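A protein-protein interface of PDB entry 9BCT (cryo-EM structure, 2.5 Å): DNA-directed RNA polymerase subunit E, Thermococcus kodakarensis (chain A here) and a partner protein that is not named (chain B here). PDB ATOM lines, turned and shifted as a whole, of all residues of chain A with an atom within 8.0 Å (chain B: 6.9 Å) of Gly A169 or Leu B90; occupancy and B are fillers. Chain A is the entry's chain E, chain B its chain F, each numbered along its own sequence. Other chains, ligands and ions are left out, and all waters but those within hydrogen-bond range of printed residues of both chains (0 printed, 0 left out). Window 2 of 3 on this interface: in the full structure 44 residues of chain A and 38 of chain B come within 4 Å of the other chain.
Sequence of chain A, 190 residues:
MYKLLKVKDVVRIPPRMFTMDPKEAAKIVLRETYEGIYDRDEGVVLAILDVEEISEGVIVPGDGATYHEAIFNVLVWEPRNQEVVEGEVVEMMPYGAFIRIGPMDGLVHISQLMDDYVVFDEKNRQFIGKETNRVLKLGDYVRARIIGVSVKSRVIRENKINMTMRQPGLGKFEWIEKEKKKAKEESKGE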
ATOM      1  N   VAL A  84       1.598  -1.082  -8.387  1.00  0.00           N
ATOM      2  CA  VAL A  84       2.035   0.296  -8.579  1.00  0.00           C
ATOM      3  C   VAL A  84       2.804   0.400  -9.887  1.00  0.00           C
ATOM      4  O   VAL A  84       3.530  -0.523 -10.273  1.00  0.00           O
ATOM      5  CB  VAL A  84       2.890   0.768  -7.387  1.00  0.00           C
ATOM      6  CG1 VAL A  84       3.020   2.285  -7.385  1.00  0.00           C
ATOM      7  CG2 VAL A  84       2.292   0.279  -6.078  1.00  0.00           C
ATOM      8  N   ARG A 143       2.690   8.540 -10.542  1.00  0.00           N
ATOM      9  CA  ARG A 143       2.791   7.172 -10.051  1.00  0.00           C
ATOM     10  C   ARG A 143       1.477   6.786  -9.391  1.00  0.00           C
ATOM     11  O   ARG A 143       0.973   7.524  -8.539  1.00  0.00           O
ATOM     12  CB  ARG A 143       3.951   7.025  -9.060  1.00  0.00           C
ATOM     13  CG  ARG A 143       3.796   5.873  -8.079  1.00  0.00           C
ATOM     14  CD  ARG A 143       5.036   5.706  -7.217  1.00  0.00           C
ATOM     15  NE  ARG A 143       6.231   6.214  -7.878  1.00  0.00           N
ATOM     16  CZ  ARG A 143       7.293   6.693  -7.243  1.00  0.00           C
ATOM     17  NH1 ARG A 143       7.343   6.745  -5.922  1.00  0.00           N
ATOM     18  NH2 ARG A 143       8.331   7.130  -7.951  1.00  0.00           N
ATOM     19  N   ALA A 144       0.925   5.639  -9.783  1.00  0.00           N
ATOM     20  CA  ALA A 144      -0.334   5.180  -9.212  1.00  0.00           C
ATOM     21  C   ALA A 144      -0.419   3.667  -9.338  1.00  0.00           C
ATOM     22  O   ALA A 144       0.258   3.057 -10.165  1.00  0.00           O
ATOM     23  CB  ALA A 144      -1.539   5.844  -9.890  1.00  0.00           C
ATOM     24  N   MET A 165      -5.358   6.860  -6.786  1.00  0.00           N
ATOM     25  CA  MET A 165      -4.379   7.920  -6.629  1.00  0.00           C
ATOM     26  C   MET A 165      -4.597   8.750  -5.367  1.00  0.00           C
ATOM     27  O   MET A 165      -3.663   9.428  -4.928  1.00  0.00           O
ATOM     28  CB  MET A 165      -4.409   8.816  -7.893  1.00  0.00           C
ATOM     29  CG  MET A 165      -3.564  10.075  -7.875  1.00  0.00           C
ATOM     30  SD  MET A 165      -2.085   9.916  -8.886  1.00  0.00           S
ATOM     31  CE  MET A 165      -2.583  10.829 -10.343  1.00  0.00           C
ATOM     32  N   ARG A 166      -5.761   8.646  -4.718  1.00  0.00           N
ATOM     33  CA  ARG A 166      -6.039   9.417  -3.512  1.00  0.00           C
ATOM     34  C   ARG A 166      -5.183   9.007  -2.322  1.00  0.00           C
ATOM     35  O   ARG A 166      -5.118   9.757  -1.342  1.00  0.00           O
ATOM     36  CB  ARG A 166      -7.512   9.291  -3.115  1.00  0.00           C
ATOM     37  CG  ARG A 166      -8.383  10.477  -3.483  1.00  0.00           C
ATOM     38  CD  ARG A 166      -9.736  10.380  -2.801  1.00  0.00           C
ATOM     39  NE  ARG A 166     -10.162  11.658  -2.241  1.00  0.00           N
ATOM     40  CZ  ARG A 166     -11.213  12.346  -2.667  1.00  0.00           C
ATOM     41  NH1 ARG A 166     -11.969  11.910  -3.661  1.00  0.00           N
ATOM     42  NH2 ARG A 166     -11.511  13.502  -2.084  1.00  0.00           N
ATOM     43  N   GLN A 167      -4.549   7.837  -2.373  1.00  0.00           N
ATOM     44  CA  GLN A 167      -3.698   7.414  -1.278  1.00  0.00           C
ATOM     45  C   GLN A 167      -2.443   8.284  -1.215  1.00  0.00           C
ATOM     46  O   GLN A 167      -1.954   8.757  -2.244  1.00  0.00           O
ATOM     47  CB  GLN A 167      -3.308   5.949  -1.444  1.00  0.00           C
ATOM     48  CG  GLN A 167      -4.336   5.111  -2.186  1.00  0.00           C
ATOM     49  CD  GLN A 167      -3.998   3.635  -2.179  1.00  0.00           C
ATOM     50  OE1 GLN A 167      -4.257   2.931  -1.202  1.00  0.00           O
ATOM     51  NE2 GLN A 167      -3.417   3.156  -3.272  1.00  0.00           N
ATOM     52  N   PRO A 168      -1.912   8.523  -0.017  1.00  0.00           N
ATOM     53  CA  PRO A 168      -0.677   9.304   0.100  1.00  0.00           C
ATOM     54  C   PRO A 168       0.504   8.571  -0.517  1.00  0.00           C
ATOM     55  O   PRO A 168       0.524   7.344  -0.631  1.00  0.00           O
ATOM     56  CB  PRO A 168      -0.496   9.471   1.614  1.00  0.00           C
ATOM     57  CG  PRO A 168      -1.842   9.185   2.204  1.00  0.00           C
ATOM     58  CD  PRO A 168      -2.471   8.175   1.299  1.00  0.00           C
ATOM     59  N   GLY A 169       1.499   9.355  -0.926  1.00  0.00           N
ATOM     60  CA  GLY A 169       2.672   8.823  -1.582  1.00  0.00           C
ATOM     61  C   GLY A 169       2.558   8.675  -3.083  1.00  0.00           C
ATOM     62  O   GLY A 169       3.528   8.246  -3.722  1.00  0.00           O
ATOM     63  N   LEU A 170       1.413   9.012  -3.666  1.00  0.00           N
ATOM     64  CA  LEU A 170       1.194   8.946  -5.101  1.00  0.00           C
ATOM     65  C   LEU A 170       1.058  10.358  -5.665  1.00  0.00           C
ATOM     66  O   LEU A 170       1.076  11.353  -4.935  1.00  0.00           O
ATOM     67  CB  LEU A 170      -0.041   8.100  -5.418  1.00  0.00           C
ATOM     68  CG  LEU A 170      -0.047   6.688  -4.827  1.00  0.00           C
ATOM     69  CD1 LEU A 170      -1.319   5.949  -5.210  1.00  0.00           C
ATOM     70  CD2 LEU A 170       1.182   5.915  -5.277  1.00  0.00           C
ATOM     71  N   GLY A 171       0.922  10.437  -6.980  1.00  0.00           N
ATOM     72  CA  GLY A 171       0.777  11.698  -7.670  1.00  0.00           C
ATOM     73  C   GLY A 171       1.989  12.043  -8.512  1.00  0.00           C
ATOM     74  O   GLY A 171       2.749  11.179  -8.956  1.00  0.00           O
ATOM     75  N   LYS A 172       2.166  13.343  -8.729  1.00  0.00           N
ATOM     76  CA  LYS A 172       3.283  13.831  -9.520  1.00  0.00           C
ATOM     77  C   LYS A 172       4.602  13.610  -8.783  1.00  0.00           C
ATOM     78  O   LYS A 172       4.645  13.463  -7.559  1.00  0.00           O
ATOM     79  CB  LYS A 172       3.106  15.315  -9.842  1.00  0.00           C
ATOM     80  CG  LYS A 172       3.541  15.705 -11.245  1.00  0.00           C
ATOM     81  CD  LYS A 172       4.048  17.137 -11.289  1.00  0.00           C
ATOM     82  CE  LYS A 172       2.934  18.135 -11.014  1.00  0.00           C
ATOM     83  NZ  LYS A 172       1.663  17.756 -11.690  1.00  0.00           N
ATOM     84  N   PHE A 173       5.690  13.578  -9.558  1.00  0.00           N
ATOM     85  CA  PHE A 173       7.014  13.404  -8.970  1.00  0.00           C
ATOM     86  C   PHE A 173       7.369  14.573  -8.059  1.00  0.00           C
ATOM     87  O   PHE A 173       7.979  14.382  -7.000  1.00  0.00           O
ATOM     88  CB  PHE A 173       8.062  13.241 -10.071  1.00  0.00           C
ATOM     89  CG  PHE A 173       8.180  11.837 -10.599  1.00  0.00           C
ATOM     90  CD1 PHE A 173       7.277  10.857 -10.217  1.00  0.00           C
ATOM     91  CD2 PHE A 173       9.195  11.498 -11.478  1.00  0.00           C
ATOM     92  CE1 PHE A 173       7.384   9.567 -10.703  1.00  0.00           C
ATOM     93  CE2 PHE A 173       9.308  10.209 -11.967  1.00  0.00           C
ATOM     94  CZ  PHE A 173       8.402   9.244 -11.578  1.00  0.00           C
ATOM     95  N   TRP A 175       5.166  16.322  -6.421  1.00  0.00           N
ATOM     96  CA  TRP A 175       4.347  16.117  -5.229  1.00  0.00           C
ATOM     97  C   TRP A 175       4.994  15.112  -4.283  1.00  0.00           C
ATOM     98  O   TRP A 175       4.995  15.308  -3.061  1.00  0.00           O
ATOM     99  CB  TRP A 175       2.946  15.650  -5.625  1.00  0.00           C
ATOM    100  CG  TRP A 175       2.173  16.643  -6.444  1.00  0.00           C
ATOM    101  CD1 TRP A 175       2.524  17.933  -6.722  1.00  0.00           C
ATOM    102  CD2 TRP A 175       0.915  16.423  -7.094  1.00  0.00           C
ATOM    103  NE1 TRP A 175       1.564  18.528  -7.503  1.00  0.00           N
ATOM    104  CE2 TRP A 175       0.565  17.622  -7.746  1.00  0.00           C
ATOM    105  CE3 TRP A 175       0.051  15.327  -7.187  1.00  0.00           C
ATOM    106  CZ2 TRP A 175      -0.610  17.757  -8.481  1.00  0.00           C
ATOM    107  CZ3 TRP A 175      -1.116  15.464  -7.917  1.00  0.00           C
ATOM    108  CH2 TRP A 175      -1.435  16.669  -8.554  1.00  0.00           C
ATOM    109  N   ILE A 176       5.552  14.030  -4.832  1.00  0.00           N
ATOM    110  CA  ILE A 176       6.234  13.035  -4.008  1.00  0.00           C
ATOM    111  C   ILE A 176       7.468  13.642  -3.351  1.00  0.00           C
ATOM    112  O   ILE A 176       7.755  13.384  -2.176  1.00  0.00           O
ATOM    113  CB  ILE A 176       6.586  11.795  -4.851  1.00  0.00           C
ATOM    114  CG1 ILE A 176       5.310  11.130  -5.374  1.00  0.00           C
ATOM    115  CG2 ILE A 176       7.410  10.804  -4.041  1.00  0.00           C
ATOM    116  CD1 ILE A 176       5.551   9.815  -6.084  1.00  0.00           C
ATOM    117  N   GLU A 177       8.218  14.456  -4.101  1.00  0.00           N
ATOM    118  CA  GLU A 177       9.393  15.113  -3.535  1.00  0.00           C
ATOM    119  C   GLU A 177       9.008  16.072  -2.414  1.00  0.00           C
ATOM    120  O   GLU A 177       9.695  16.146  -1.387  1.00  0.00           O
ATOM    121  CB  GLU A 177      10.159  15.852  -4.633  1.00  0.00           C
ATOM    122  CG  GLU A 177      10.964  14.944  -5.547  1.00  0.00           C
ATOM    123  CD  GLU A 177      12.023  14.155  -4.802  1.00  0.00           C
ATOM    124  OE1 GLU A 177      13.103  14.719  -4.527  1.00  0.00           O
ATOM    125  OE2 GLU A 177      11.776  12.971  -4.492  1.00  0.00           O
ATOM    126  N   LYS A 178       7.917  16.820  -2.595  1.00  0.00           N
ATOM    127  CA  LYS A 178       7.461  17.738  -1.556  1.00  0.00           C
ATOM    128  C   LYS A 178       6.980  16.985  -0.321  1.00  0.00           C
ATOM    129  O   LYS A 178       7.217  17.422   0.811  1.00  0.00           O
ATOM    130  CB  LYS A 178       6.357  18.642  -2.102  1.00  0.00           C
ATOM    131  CG  LYS A 178       6.868  19.927  -2.742  1.00  0.00           C
ATOM    132  CD  LYS A 178       5.939  20.441  -3.839  1.00  0.00           C
ATOM    133  CE  LYS A 178       4.476  20.131  -3.548  1.00  0.00           C
ATOM    134  NZ  LYS A 178       3.619  20.328  -4.749  1.00  0.00           N
ATOM    135  N   GLU A 179       6.289  15.858  -0.519  1.00  0.00           N
ATOM    136  CA  GLU A 179       5.861  15.042   0.614  1.00  0.00           C
ATOM    137  C   GLU A 179       7.057  14.457   1.356  1.00  0.00           C
ATOM    138  O   GLU A 179       7.046  14.369   2.590  1.00  0.00           O
ATOM    139  CB  GLU A 179       4.928  13.929   0.136  1.00  0.00           C
ATOM    140  CG  GLU A 179       3.460  14.322   0.107  1.00  0.00           C
ATOM    141  CD  GLU A 179       2.775  13.921  -1.185  1.00  0.00           C
ATOM    142  OE1 GLU A 179       3.350  13.105  -1.936  1.00  0.00           O
ATOM    143  OE2 GLU A 179       1.662  14.421  -1.449  1.00  0.00           O
ATOM    144  N   LYS A 180       8.092  14.046   0.620  1.00  0.00           N
ATOM    145  CA  LYS A 180       9.302  13.529   1.248  1.00  0.00           C
ATOM    146  C   LYS A 180      10.033  14.613   2.033  1.00  0.00           C
ATOM    147  O   LYS A 180      10.639  14.324   3.072  1.00  0.00           O
ATOM    148  CB  LYS A 180      10.215  12.917   0.182  1.00  0.00           C
ATOM    149  CG  LYS A 180      11.605  12.529   0.666  1.00  0.00           C
ATOM    150  CD  LYS A 180      12.631  12.645  -0.450  1.00  0.00           C
ATOM    151  CE  LYS A 180      12.635  14.038  -1.059  1.00  0.00           C
ATOM    152  NZ  LYS A 180      12.832  15.095  -0.028  1.00  0.00           N
ATOM    153  N   LYS A 181       9.977  15.861   1.558  1.00  0.00           N
ATOM    154  CA  LYS A 181      10.627  16.960   2.265  1.00  0.00           C
ATOM    155  C   LYS A 181      10.014  17.174   3.644  1.00  0.00           C
ATOM    156  O   LYS A 181      10.732  17.447   4.615  1.00  0.00           O
ATOM    157  CB  LYS A 181      10.537  18.239   1.430  1.00  0.00           C
ATOM    158  CG  LYS A 181      11.099  19.481   2.110  1.00  0.00           C
ATOM    159  CD  LYS A 181       9.998  20.470   2.464  1.00  0.00           C
ATOM    160  CE  LYS A 181       9.083  20.738   1.281  1.00  0.00           C
ATOM    161  NZ  LYS A 181       7.843  21.455   1.687  1.00  0.00           N
ATOM    162  N   ALA A 183       8.574  14.858   5.500  1.00  0.00           N
ATOM    163  CA  ALA A 183       8.984  13.728   6.325  1.00  0.00           C
ATOM    164  C   ALA A 183      10.484  13.764   6.594  1.00  0.00           C
ATOM    165  O   ALA A 183      11.217  14.541   5.981  1.00  0.00           O
ATOM    166  CB  ALA A 183       8.595  12.417   5.660  1.00  0.00           C
ATOM    167  N   GLU B  87      13.711   5.396  -2.599  1.00  0.00           N
ATOM    168  CA  GLU B  87      14.733   6.164  -1.904  1.00  0.00           C
ATOM    169  C   GLU B  87      14.499   6.303  -0.409  1.00  0.00           C
ATOM    170  O   GLU B  87      15.455   6.587   0.319  1.00  0.00           O
ATOM    171  CB  GLU B  87      14.853   7.572  -2.512  1.00  0.00           C
ATOM    172  CG  GLU B  87      13.557   8.366  -2.501  1.00  0.00           C
ATOM    173  CD  GLU B  87      12.789   8.245  -3.803  1.00  0.00           C
ATOM    174  OE1 GLU B  87      13.419   7.960  -4.843  1.00  0.00           O
ATOM    175  OE2 GLU B  87      11.554   8.437  -3.786  1.00  0.00           O
ATOM    176  N   ASP B  88      13.274   6.114   0.069  1.00  0.00           N
ATOM    177  CA  ASP B  88      12.968   6.276   1.485  1.00  0.00           C
ATOM    178  C   ASP B  88      11.841   5.309   1.840  1.00  0.00           C
ATOM    179  O   ASP B  88      11.569   4.358   1.103  1.00  0.00           O
ATOM    180  CB  ASP B  88      12.633   7.745   1.795  1.00  0.00           C
ATOM    181  CG  ASP B  88      11.313   8.182   1.197  1.00  0.00           C
ATOM    182  OD1 ASP B  88      11.298   8.594   0.018  1.00  0.00           O
ATOM    183  OD2 ASP B  88      10.292   8.117   1.909  1.00  0.00           O
ATOM    184  N   TYR B  89      11.197   5.541   2.985  1.00  0.00           N
ATOM    185  CA  TYR B  89      10.157   4.640   3.466  1.00  0.00           C
ATOM    186  C   TYR B  89       8.799   4.882   2.816  1.00  0.00           C
ATOM    187  O   TYR B  89       7.964   3.972   2.817  1.00  0.00           O
ATOM    188  CB  TYR B  89      10.022   4.761   4.986  1.00  0.00           C
ATOM    189  CG  TYR B  89       9.795   3.447   5.703  1.00  0.00           C
ATOM    190  CD1 TYR B  89       9.323   2.331   5.023  1.00  0.00           C
ATOM    191  CD2 TYR B  89      10.045   3.326   7.064  1.00  0.00           C
ATOM    192  CE1 TYR B  89       9.110   1.132   5.676  1.00  0.00           C
ATOM    193  CE2 TYR B  89       9.835   2.129   7.725  1.00  0.00           C
ATOM    194  CZ  TYR B  89       9.368   1.037   7.026  1.00  0.00           C
ATOM    195  OH  TYR B  89       9.155  -0.157   7.676  1.00  0.00           O
ATOM    196  N   LEU B  90       8.552   6.077   2.272  1.00  0.00           N
ATOM    197  CA  LEU B  90       7.214   6.404   1.780  1.00  0.00           C
ATOM    198  C   LEU B  90       6.818   5.528   0.596  1.00  0.00           C
ATOM    199  O   LEU B  90       5.755   4.897   0.608  1.00  0.00           O
ATOM    200  CB  LEU B  90       7.141   7.884   1.401  1.00  0.00           C
ATOM    201  CG  LEU B  90       5.811   8.365   0.817  1.00  0.00           C
ATOM    202  CD1 LEU B  90       4.694   8.228   1.840  1.00  0.00           C
ATOM    203  CD2 LEU B  90       5.925   9.802   0.333  1.00  0.00           C
ATOM    204  N   ASP B  91       7.665   5.470  -0.436  1.00  0.00           N
ATOM    205  CA  ASP B  91       7.321   4.688  -1.619  1.00  0.00           C
ATOM    206  C   ASP B  91       7.325   3.193  -1.328  1.00  0.00           C
ATOM    207  O   ASP B  91       6.494   2.457  -1.869  1.00  0.00           O
ATOM    208  CB  ASP B  91       8.273   5.022  -2.768  1.00  0.00           C
ATOM    209  CG  ASP B  91       9.706   5.181  -2.311  1.00  0.00           C
ATOM    210  OD1 ASP B  91      10.024   4.741  -1.189  1.00  0.00           O
ATOM    211  OD2 ASP B  91      10.511   5.758  -3.070  1.00  0.00           O
ATOM    212  N   ILE B  92       8.231   2.732  -0.462  1.00  0.00           N
ATOM    213  CA  ILE B  92       8.224   1.331  -0.049  1.00  0.00           C
ATOM    214  C   ILE B  92       6.914   0.992   0.653  1.00  0.00           C
ATOM    215  O   ILE B  92       6.315  -0.065   0.410  1.00  0.00           O
ATOM    216  CB  ILE B  92       9.447   1.036   0.843  1.00  0.00           C
ATOM    217  CG1 ILE B  92      10.701   0.852  -0.015  1.00  0.00           C
ATOM    218  CG2 ILE B  92       9.209  -0.189   1.718  1.00  0.00           C
ATOM    219  CD1 ILE B  92      10.754  -0.471  -0.750  1.00  0.00           C
ATOM    220  N   ARG B  93       6.445   1.888   1.525  1.00  0.00           N
ATOM    221  CA  ARG B  93       5.187   1.660   2.228  1.00  0.00           C
ATOM    222  C   ARG B  93       4.003   1.642   1.268  1.00  0.00           C
ATOM    223  O   ARG B  93       3.134   0.770   1.368  1.00  0.00           O
ATOM    224  CB  ARG B  93       4.987   2.726   3.304  1.00  0.00           C
ATOM    225  CG  ARG B  93       3.702   2.569   4.102  1.00  0.00           C
ATOM    226  CD  ARG B  93       3.665   3.520   5.286  1.00  0.00           C
ATOM    227  NE  ARG B  93       4.987   3.725   5.866  1.00  0.00           N
ATOM    228  CZ  ARG B  93       5.535   2.935   6.780  1.00  0.00           C
ATOM    229  NH1 ARG B  93       4.900   1.869   7.242  1.00  0.00           N
ATOM    230  NH2 ARG B  93       6.749   3.220   7.240  1.00  0.00           N
ATOM    231  N   VAL B  94       3.947   2.592   0.329  1.00  0.00           N
ATOM    232  CA  VAL B  94       2.824   2.599  -0.608  1.00  0.00           C
ATOM    233  C   VAL B  94       2.919   1.462  -1.617  1.00  0.00           C
ATOM    234  O   VAL B  94       1.923   1.143  -2.276  1.00  0.00           O
ATOM    235  CB  VAL B  94       2.686   3.952  -1.335  1.00  0.00           C
ATOM    236  CG1 VAL B  94       2.817   5.102  -0.355  1.00  0.00           C
ATOM    237  CG2 VAL B  94       3.710   4.073  -2.453  1.00  0.00           C
ATOM    238  N   ILE B  95       4.089   0.840  -1.763  1.00  0.00           N
ATOM    239  CA  ILE B  95       4.186  -0.347  -2.605  1.00  0.00           C
ATOM    240  C   ILE B  95       3.723  -1.587  -1.847  1.00  0.00           C
ATOM    241  O   ILE B  95       2.957  -2.401  -2.376  1.00  0.00           O
ATOM    242  CB  ILE B  95       5.626  -0.504  -3.133  1.00  0.00           C
ATOM    243  CG1 ILE B  95       5.860   0.421  -4.328  1.00  0.00           C
ATOM    244  CG2 ILE B  95       5.914  -1.948  -3.520  1.00  0.00           C
ATOM    245  CD1 ILE B  95       7.321   0.710  -4.595  1.00  0.00           C
ATOM    246  N   ILE B 112      16.811  -0.136   0.742  1.00  0.00           N
ATOM    247  CA  ILE B 112      17.048   1.220   0.250  1.00  0.00           C
ATOM    248  C   ILE B 112      18.507   1.410  -0.160  1.00  0.00           C
ATOM    249  O   ILE B 112      18.790   1.876  -1.273  1.00  0.00           O
ATOM    250  CB  ILE B 112      16.607   2.254   1.301  1.00  0.00           C
ATOM    251  CG1 ILE B 112      15.096   2.478   1.216  1.00  0.00           C
ATOM    252  CG2 ILE B 112      17.348   3.576   1.113  1.00  0.00           C
ATOM    253  CD1 ILE B 112      14.479   2.982   2.497  1.00  0.00           C
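N of Glu B87 is in hydrogen-bond range of OD2 of Asp B91. The side-chain carboxylate of Asp B88 lies within hydrogen-bond range of the backbone NH of Leu B90 (2.7 Å). The backbone NH of Arg A143 is in hydrogen-bond range of the backbone carbonyl oxygen of Gly A171.
CG2 of Val A84 touches O of Val B94, at 3.9 Å. Val A84 touches Ile B95. NH1 of Arg A143 touches CB of Asp B91, at 3.7 Å. Pro A168 touches Val B94 (O to CG1, 3.2 Å). Leu B90 touches Gly A169 (CD2 to CA, 3.9 Å). Gly A169 touches Val B94. CG of Lys A180 touches OD1 of Asp B88 (3.9998 Å).
Of chain A, only Gly A169 (3.9 Å) comes within 4 Å of Leu B90. Printed residues of chain A within 4 Å of Ile B95: Val A84 (3.98 Å). Printed residues of chain A within 4 Å of Asp B88: Lys A180 (3.9998 Å). Printed residues of chain A within 4 Å of Val B94: Val A84, Pro A168 and Gly A169. Of the printed residues of chain B, Arg A143 touches Asp B91. Of the printed residues of chain B, Val A84 touches Val B94 (3.9 Å) and Ile B95 (3.98 Å). Leu A170 touches none of the printed residues of chain B. Lys A181 touches none of the printed residues of chain B. The nearest residue of chain B that does not touch Gly A169 is Asp B91 (5.6 Å). The nearest residue of chain A that does not touch Leu B90 is Glu A179 (4.3 Å).
Hydrophobic or aromatic side chains of chain B within 4 Å of the printed part of chain A: Leu B90, Val B94 and Ile B95. Of the 20 printed residues of chain A, 5 touch a printed residue of chain B. Hydrophobic or aromatic side chains of chain A within 4 Å of the printed part of chain B: Val A84. Along chain A the printed residues that touch a printed residue of chain B span positions 84 to 180. Among the printed residues, 7 pairs touch across the chains.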
